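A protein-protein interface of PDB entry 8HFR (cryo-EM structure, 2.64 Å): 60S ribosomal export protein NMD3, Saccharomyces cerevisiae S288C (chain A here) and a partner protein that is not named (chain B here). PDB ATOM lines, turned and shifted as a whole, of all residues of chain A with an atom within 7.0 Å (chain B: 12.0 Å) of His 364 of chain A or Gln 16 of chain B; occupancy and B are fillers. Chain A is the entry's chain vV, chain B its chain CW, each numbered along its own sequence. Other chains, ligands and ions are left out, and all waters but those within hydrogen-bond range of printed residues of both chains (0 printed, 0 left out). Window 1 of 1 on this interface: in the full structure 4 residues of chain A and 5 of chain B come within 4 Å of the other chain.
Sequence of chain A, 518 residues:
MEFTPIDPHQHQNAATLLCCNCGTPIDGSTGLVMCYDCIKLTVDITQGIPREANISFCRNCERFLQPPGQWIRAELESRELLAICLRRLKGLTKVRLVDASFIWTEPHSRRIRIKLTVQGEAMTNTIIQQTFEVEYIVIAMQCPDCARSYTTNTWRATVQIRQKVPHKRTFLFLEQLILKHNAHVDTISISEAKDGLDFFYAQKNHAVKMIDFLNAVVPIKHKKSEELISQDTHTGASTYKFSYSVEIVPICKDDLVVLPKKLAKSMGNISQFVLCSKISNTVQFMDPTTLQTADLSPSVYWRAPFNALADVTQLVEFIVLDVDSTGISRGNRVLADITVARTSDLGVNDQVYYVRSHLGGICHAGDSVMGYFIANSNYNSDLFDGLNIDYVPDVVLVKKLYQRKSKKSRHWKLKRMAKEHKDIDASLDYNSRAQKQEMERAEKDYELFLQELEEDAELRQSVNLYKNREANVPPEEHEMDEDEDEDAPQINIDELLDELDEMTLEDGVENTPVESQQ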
ATOM      1  N   VAL A 320     -21.230  10.836  21.001  1.00  0.00           N
ATOM      2  CA  VAL A 320     -22.530  11.277  21.497  1.00  0.00           C
ATOM      3  C   VAL A 320     -23.054  10.267  22.509  1.00  0.00           C
ATOM      4  O   VAL A 320     -23.233   9.085  22.193  1.00  0.00           O
ATOM      5  CB  VAL A 320     -23.517  11.474  20.343  1.00  0.00           C
ATOM      6  CG1 VAL A 320     -24.818  12.056  20.855  1.00  0.00           C
ATOM      7  CG2 VAL A 320     -22.912  12.370  19.298  1.00  0.00           C
ATOM      8  N   LEU A 321     -23.308  10.732  23.728  1.00  0.00           N
ATOM      9  CA  LEU A 321     -23.815   9.869  24.787  1.00  0.00           C
ATOM     10  C   LEU A 321     -25.338   9.882  24.861  1.00  0.00           C
ATOM     11  O   LEU A 321     -25.959   8.821  24.957  1.00  0.00           O
ATOM     12  CB  LEU A 321     -23.227  10.285  26.138  1.00  0.00           C
ATOM     13  CG  LEU A 321     -21.741  10.013  26.347  1.00  0.00           C
ATOM     14  CD1 LEU A 321     -21.256  10.691  27.606  1.00  0.00           C
ATOM     15  CD2 LEU A 321     -21.482   8.526  26.412  1.00  0.00           C
ATOM     16  N   ASP A 322     -25.955  11.060  24.829  1.00  0.00           N
ATOM     17  CA  ASP A 322     -27.400  11.124  25.004  1.00  0.00           C
ATOM     18  C   ASP A 322     -27.956  12.336  24.276  1.00  0.00           C
ATOM     19  O   ASP A 322     -27.263  13.331  24.065  1.00  0.00           O
ATOM     20  CB  ASP A 322     -27.786  11.178  26.484  1.00  0.00           C
ATOM     21  CG  ASP A 322     -29.081  10.460  26.770  1.00  0.00           C
ATOM     22  OD1 ASP A 322     -29.750  10.024  25.813  1.00  0.00           O
ATOM     23  OD2 ASP A 322     -29.431  10.318  27.954  1.00  0.00           O
ATOM     24  N   VAL A 323     -29.230  12.234  23.890  1.00  0.00           N
ATOM     25  CA  VAL A 323     -29.923  13.250  23.110  1.00  0.00           C
ATOM     26  C   VAL A 323     -31.174  13.671  23.888  1.00  0.00           C
ATOM     27  O   VAL A 323     -31.758  12.887  24.635  1.00  0.00           O
ATOM     28  CB  VAL A 323     -30.268  12.713  21.686  1.00  0.00           C
ATOM     29  CG1 VAL A 323     -30.943  13.750  20.778  1.00  0.00           C
ATOM     30  CG2 VAL A 323     -29.028  12.174  20.990  1.00  0.00           C
ATOM     31  N   LEU A 359     -27.668  19.950  15.726  1.00  0.00           N
ATOM     32  CA  LEU A 359     -27.551  18.579  15.237  1.00  0.00           C
ATOM     33  C   LEU A 359     -28.409  17.646  16.091  1.00  0.00           C
ATOM     34  O   LEU A 359     -27.926  16.737  16.759  1.00  0.00           O
ATOM     35  CB  LEU A 359     -26.088  18.142  15.228  1.00  0.00           C
ATOM     36  CG  LEU A 359     -25.086  18.859  14.316  1.00  0.00           C
ATOM     37  CD1 LEU A 359     -23.917  17.939  14.014  1.00  0.00           C
ATOM     38  CD2 LEU A 359     -25.717  19.346  13.024  1.00  0.00           C
ATOM     39  N   GLY A 360     -29.713  17.895  16.066  1.00  0.00           N
ATOM     40  CA  GLY A 360     -30.628  17.088  16.842  1.00  0.00           C
ATOM     41  C   GLY A 360     -31.390  16.079  16.018  1.00  0.00           C
ATOM     42  O   GLY A 360     -31.544  14.925  16.422  1.00  0.00           O
ATOM     43  N   GLY A 361     -31.872  16.502  14.854  1.00  0.00           N
ATOM     44  CA  GLY A 361     -32.552  15.573  13.979  1.00  0.00           C
ATOM     45  C   GLY A 361     -31.643  14.619  13.245  1.00  0.00           C
ATOM     46  O   GLY A 361     -32.111  13.589  12.754  1.00  0.00           O
ATOM     47  N   ILE A 362     -30.350  14.929  13.181  1.00  0.00           N
ATOM     48  CA  ILE A 362     -29.413  14.165  12.371  1.00  0.00           C
ATOM     49  C   ILE A 362     -28.589  13.177  13.193  1.00  0.00           C
ATOM     50  O   ILE A 362     -28.017  12.240  12.613  1.00  0.00           O
ATOM     51  CB  ILE A 362     -28.494  15.126  11.582  1.00  0.00           C
ATOM     52  CG1 ILE A 362     -28.066  14.515  10.256  1.00  0.00           C
ATOM     53  CG2 ILE A 362     -27.269  15.547  12.379  1.00  0.00           C
ATOM     54  CD1 ILE A 362     -29.179  14.440   9.294  1.00  0.00           C
ATOM     55  N   CYS A 363     -28.533  13.333  14.516  1.00  0.00           N
ATOM     56  CA  CYS A 363     -27.633  12.563  15.365  1.00  0.00           C
ATOM     57  C   CYS A 363     -28.412  11.698  16.345  1.00  0.00           C
ATOM     58  O   CYS A 363     -29.442  12.119  16.881  1.00  0.00           O
ATOM     59  CB  CYS A 363     -26.691  13.482  16.149  1.00  0.00           C
ATOM     60  SG  CYS A 363     -25.359  14.221  15.187  1.00  0.00           S
ATOM     61  N   HIS A 364     -27.902  10.490  16.584  1.00  0.00           N
ATOM     62  CA  HIS A 364     -28.438   9.573  17.576  1.00  0.00           C
ATOM     63  C   HIS A 364     -27.293   9.078  18.440  1.00  0.00           C
ATOM     64  O   HIS A 364     -26.132   9.144  18.035  1.00  0.00           O
ATOM     65  CB  HIS A 364     -29.162   8.399  16.913  1.00  0.00           C
ATOM     66  CG  HIS A 364     -29.931   8.796  15.696  1.00  0.00           C
ATOM     67  ND1 HIS A 364     -29.452   8.601  14.420  1.00  0.00           N
ATOM     68  CD2 HIS A 364     -31.123   9.420  15.561  1.00  0.00           C
ATOM     69  CE1 HIS A 364     -30.326   9.072  13.549  1.00  0.00           C
ATOM     70  NE2 HIS A 364     -31.349   9.574  14.214  1.00  0.00           N
ATOM     71  N   ALA A 365     -27.631   8.571  19.625  1.00  0.00           N
ATOM     72  CA  ALA A 365     -26.630   8.283  20.648  1.00  0.00           C
ATOM     73  C   ALA A 365     -25.710   7.136  20.250  1.00  0.00           C
ATOM     74  O   ALA A 365     -26.166   6.063  19.850  1.00  0.00           O
ATOM     75  CB  ALA A 365     -27.319   7.956  21.972  1.00  0.00           C
ATOM     76  N   GLY A 366     -24.404   7.378  20.353  1.00  0.00           N
ATOM     77  CA  GLY A 366     -23.400   6.353  20.155  1.00  0.00           C
ATOM     78  C   GLY A 366     -22.440   6.577  19.008  1.00  0.00           C
ATOM     79  O   GLY A 366     -21.587   5.716  18.769  1.00  0.00           O
ATOM     80  N   ASP A 367     -22.528   7.696  18.292  1.00  0.00           N
ATOM     81  CA  ASP A 367     -21.651   7.888  17.147  1.00  0.00           C
ATOM     82  C   ASP A 367     -20.743   9.108  17.286  1.00  0.00           C
ATOM     83  O   ASP A 367     -20.697   9.750  18.342  1.00  0.00           O
ATOM     84  CB  ASP A 367     -22.480   7.951  15.861  1.00  0.00           C
ATOM     85  CG  ASP A 367     -23.539   9.037  15.881  1.00  0.00           C
ATOM     86  OD1 ASP A 367     -23.647   9.779  16.878  1.00  0.00           O
ATOM     87  OD2 ASP A 367     -24.289   9.130  14.886  1.00  0.00           O
ATOM     88  N   SER A 368     -20.025   9.434  16.219  1.00  0.00           N
ATOM     89  CA  SER A 368     -18.937  10.396  16.265  1.00  0.00           C
ATOM     90  C   SER A 368     -19.308  11.660  15.505  1.00  0.00           C
ATOM     91  O   SER A 368     -19.884  11.595  14.414  1.00  0.00           O
ATOM     92  CB  SER A 368     -17.663   9.785  15.686  1.00  0.00           C
ATOM     93  OG  SER A 368     -16.588  10.695  15.750  1.00  0.00           O
ATOM     94  N   LYS A 400     -21.407  15.499  11.275  1.00  0.00           N
ATOM     95  CA  LYS A 400     -21.378  14.082  11.589  1.00  0.00           C
ATOM     96  C   LYS A 400     -20.675  13.329  10.468  1.00  0.00           C
ATOM     97  O   LYS A 400     -20.846  13.651   9.289  1.00  0.00           O
ATOM     98  CB  LYS A 400     -22.805  13.561  11.784  1.00  0.00           C
ATOM     99  CG  LYS A 400     -22.938  12.097  12.118  1.00  0.00           C
ATOM    100  CD  LYS A 400     -24.399  11.693  12.117  1.00  0.00           C
ATOM    101  CE  LYS A 400     -24.574  10.255  11.680  1.00  0.00           C
ATOM    102  NZ  LYS A 400     -26.006   9.916  11.497  1.00  0.00           N
ATOM    103  N   GLY B   8     -24.153  -4.470  16.015  1.00  0.00           N
ATOM    104  CA  GLY B   8     -25.463  -4.972  16.405  1.00  0.00           C
ATOM    105  C   GLY B   8     -26.598  -4.087  15.908  1.00  0.00           C
ATOM    106  O   GLY B   8     -27.727  -4.577  15.786  1.00  0.00           O
ATOM    107  N   ASN B   9     -26.302  -2.811  15.619  1.00  0.00           N
ATOM    108  CA  ASN B   9     -27.247  -1.805  15.113  1.00  0.00           C
ATOM    109  C   ASN B   9     -28.422  -1.600  16.073  1.00  0.00           C
ATOM    110  O   ASN B   9     -29.582  -1.856  15.751  1.00  0.00           O
ATOM    111  CB  ASN B   9     -27.737  -2.148  13.699  1.00  0.00           C
ATOM    112  N   ILE B  10     -28.090  -1.121  17.271  1.00  0.00           N
ATOM    113  CA  ILE B  10     -29.079  -0.709  18.256  1.00  0.00           C
ATOM    114  C   ILE B  10     -29.317   0.792  18.234  1.00  0.00           C
ATOM    115  O   ILE B  10     -30.033   1.311  19.095  1.00  0.00           O
ATOM    116  CB  ILE B  10     -28.654  -1.143  19.659  1.00  0.00           C
ATOM    117  N   ASN B  11     -28.748   1.490  17.259  1.00  0.00           N
ATOM    118  CA  ASN B  11     -28.767   2.947  17.204  1.00  0.00           C
ATOM    119  C   ASN B  11     -29.004   3.346  15.751  1.00  0.00           C
ATOM    120  O   ASN B  11     -29.481   2.536  14.946  1.00  0.00           O
ATOM    121  CB  ASN B  11     -27.478   3.527  17.797  1.00  0.00           C
ATOM    122  N   MET B  12     -28.691   4.609  15.435  1.00  0.00           N
ATOM    123  CA  MET B  12     -28.892   5.234  14.121  1.00  0.00           C
ATOM    124  C   MET B  12     -30.374   5.199  13.722  1.00  0.00           C
ATOM    125  O   MET B  12     -30.802   4.457  12.830  1.00  0.00           O
ATOM    126  CB  MET B  12     -27.989   4.613  13.044  1.00  0.00           C
ATOM    127  N   MET B  13     -31.148   5.988  14.479  1.00  0.00           N
ATOM    128  CA  MET B  13     -32.574   6.327  14.358  1.00  0.00           C
ATOM    129  C   MET B  13     -33.508   5.184  14.733  1.00  0.00           C
ATOM    130  O   MET B  13     -34.726   5.345  14.603  1.00  0.00           O
ATOM    131  CB  MET B  13     -32.972   6.829  12.958  1.00  0.00           C
ATOM    132  N   ALA B  14     -32.998   4.045  15.202  1.00  0.00           N
ATOM    133  CA  ALA B  14     -33.886   2.928  15.508  1.00  0.00           C
ATOM    134  C   ALA B  14     -34.531   3.091  16.877  1.00  0.00           C
ATOM    135  O   ALA B  14     -35.747   2.922  17.020  1.00  0.00           O
ATOM    136  CB  ALA B  14     -33.118   1.610  15.430  1.00  0.00           C
ATOM    137  N   GLN B  15     -33.738   3.427  17.892  1.00  0.00           N
ATOM    138  CA  GLN B  15     -34.245   3.540  19.252  1.00  0.00           C
ATOM    139  C   GLN B  15     -33.929   4.866  19.926  1.00  0.00           C
ATOM    140  O   GLN B  15     -34.730   5.317  20.753  1.00  0.00           O
ATOM    141  CB  GLN B  15     -33.696   2.402  20.124  1.00  0.00           C
ATOM    142  N   GLN B  16     -32.813   5.506  19.602  1.00  0.00           N
ATOM    143  CA  GLN B  16     -32.396   6.735  20.253  1.00  0.00           C
ATOM    144  C   GLN B  16     -32.902   7.946  19.482  1.00  0.00           C
ATOM    145  O   GLN B  16     -33.208   7.863  18.287  1.00  0.00           O
ATOM    146  CB  GLN B  16     -30.872   6.785  20.383  1.00  0.00           C
ATOM    147  N   GLN B  17     -32.973   9.079  20.199  1.00  0.00           N
ATOM    148  CA  GLN B  17     -33.494  10.361  19.707  1.00  0.00           C
ATOM    149  C   GLN B  17     -34.903  10.216  19.133  1.00  0.00           C
ATOM    150  O   GLN B  17     -35.235  10.765  18.081  1.00  0.00           O
ATOM    151  CB  GLN B  17     -32.544  11.001  18.692  1.00  0.00           C
ATOM    152  N   MET B  18     -35.739   9.453  19.835  1.00  0.00           N
ATOM    153  CA  MET B  18     -37.146   9.283  19.493  1.00  0.00           C
ATOM    154  C   MET B  18     -38.040   9.889  20.569  1.00  0.00           C
ATOM    155  O   MET B  18     -39.098   9.353  20.902  1.00  0.00           O
ATOM    156  CB  MET B  18     -37.482   7.807  19.285  1.00  0.00           C
ATOM    157  N   GLN B  19     -37.610  11.018  21.129  1.00  0.00           N
ATOM    158  CA  GLN B  19     -38.325  11.685  22.208  1.00  0.00           C
ATOM    159  C   GLN B  19     -38.460  13.176  21.942  1.00  0.00           C
ATOM    160  O   GLN B  19     -38.254  13.994  22.842  1.00  0.00           O
ATOM    161  CB  GLN B  19     -37.637  11.440  23.551  1.00  0.00           C
ATOM    162  N   GLN B  20     -38.806  13.550  20.709  1.00  0.00           N
ATOM    163  CA  GLN B  20     -39.039  14.945  20.357  1.00  0.00           C
ATOM    164  C   GLN B  20     -40.517  15.312  20.385  1.00  0.00           C
ATOM    165  O   GLN B  20     -40.962  16.146  19.585  1.00  0.00           O
ATOM    166  CB  GLN B  20     -38.437  15.249  18.984  1.00  0.00           C
ATOM    167  N   ASN B  21     -41.286  14.711  21.290  1.00  0.00           N
ATOM    168  CA  ASN B  21     -42.726  14.906  21.342  1.00  0.00           C
ATOM    169  C   ASN B  21     -43.072  16.297  21.877  1.00  0.00           C
ATOM    170  O   ASN B  21     -42.239  17.010  22.440  1.00  0.00           O
ATOM    171  CB  ASN B  21     -43.371  13.821  22.203  1.00  0.00           C
ATOM    172  N   ASN B  65     -44.576  12.751  17.129  1.00  0.00           N
ATOM    173  CA  ASN B  65     -43.436  13.291  17.867  1.00  0.00           C
ATOM    174  C   ASN B  65     -42.337  13.865  16.976  1.00  0.00           C
ATOM    175  O   ASN B  65     -41.230  14.109  17.471  1.00  0.00           O
ATOM    176  CB  ASN B  65     -42.844  12.205  18.768  1.00  0.00           C
ATOM    177  N   SER B  66     -42.601  14.082  15.690  1.00  0.00           N
ATOM    178  CA  SER B  66     -41.603  14.624  14.780  1.00  0.00           C
ATOM    179  C   SER B  66     -42.209  15.733  13.927  1.00  0.00           C
ATOM    180  O   SER B  66     -43.426  15.948  13.957  1.00  0.00           O
ATOM    181  CB  SER B  66     -41.032  13.510  13.897  1.00  0.00           C
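Among the printed residues, merely in contact across the chains: Val 323 of chain A with Gln 17 of chain B (3.8 Å), Cys 363 of chain A with Gln 17 of chain B (3.8 Å), His 364 of chain A with Met 12 of chain B (3.4 Å), His 364 of chain A with Gln 16 of chain B (3.8 Å), His 364 of chain A with Gln 17 of chain B (3.8 Å), Ala 365 of chain A with Asn 11 of chain B (3.5 Å) and Ala 365 of chain A with Gln 16 of chain B (3.8 Å).
A ring nitrogen (ND1) of His 364 of chain A is in hydrogen-bond range of the backbone NH (N) of Met 13 of chain B (3.1 Å).
Val 323 of chain A touches just one residue of chain B: Gln 17.
No residue of chain B comes within 4 Å of Gly 360 of chain A.
No residue of chain B comes within 4 Å of Gly 361 of chain A.
No residue of chain B comes within 4 Å of Ile 362 of chain A.
Of chain B, only Asn 11 (3.5 Å) and Gln 16 (3.8 Å) come within 4 Å of Ala 365 of chain A.
No residue of chain B comes within 4 Å of Gly 366 of chain A.
Printed residues of chain A within 4 Å of Asn 11 of chain B: Ala 365 (3.5 Å).
Printed residues of chain A within 4 Å of Met 12 of chain B: His 364 (3.4 Å).
Printed residues of chain A within 4 Å of Met 13 of chain B: His 364.
Gln 15 of chain B touches none of the printed residues of chain A.
Of chain A, only His 364 and Ala 365 come within 4 Å of Gln 16 of chain B.
Printed residues of chain A within 4 Å of Gln 17 of chain B: Val 323 (3.8 Å), Cys 363 (3.8 Å) and His 364 (3.8 Å).
The nearest residue of chain B that does not touch His 364 of chain A is Asn 11 of chain B (5.2 Å).
Hydrophobic or aromatic side chains of chain A within 4 Å of the printed part of chain B: Val 323 and His 364.
Of the 16 printed residues of chain B, 5 touch a printed residue of chain A.
Printed residues of chain B that touch a printed residue of chain A: Asn 11, Met 12, Met 13, Gln 16 and Gln 17.
Among the printed residues, no Asp or Glu carboxylate lies within 4 Å of a Lys or Arg side-chain nitrogen of the other chain.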
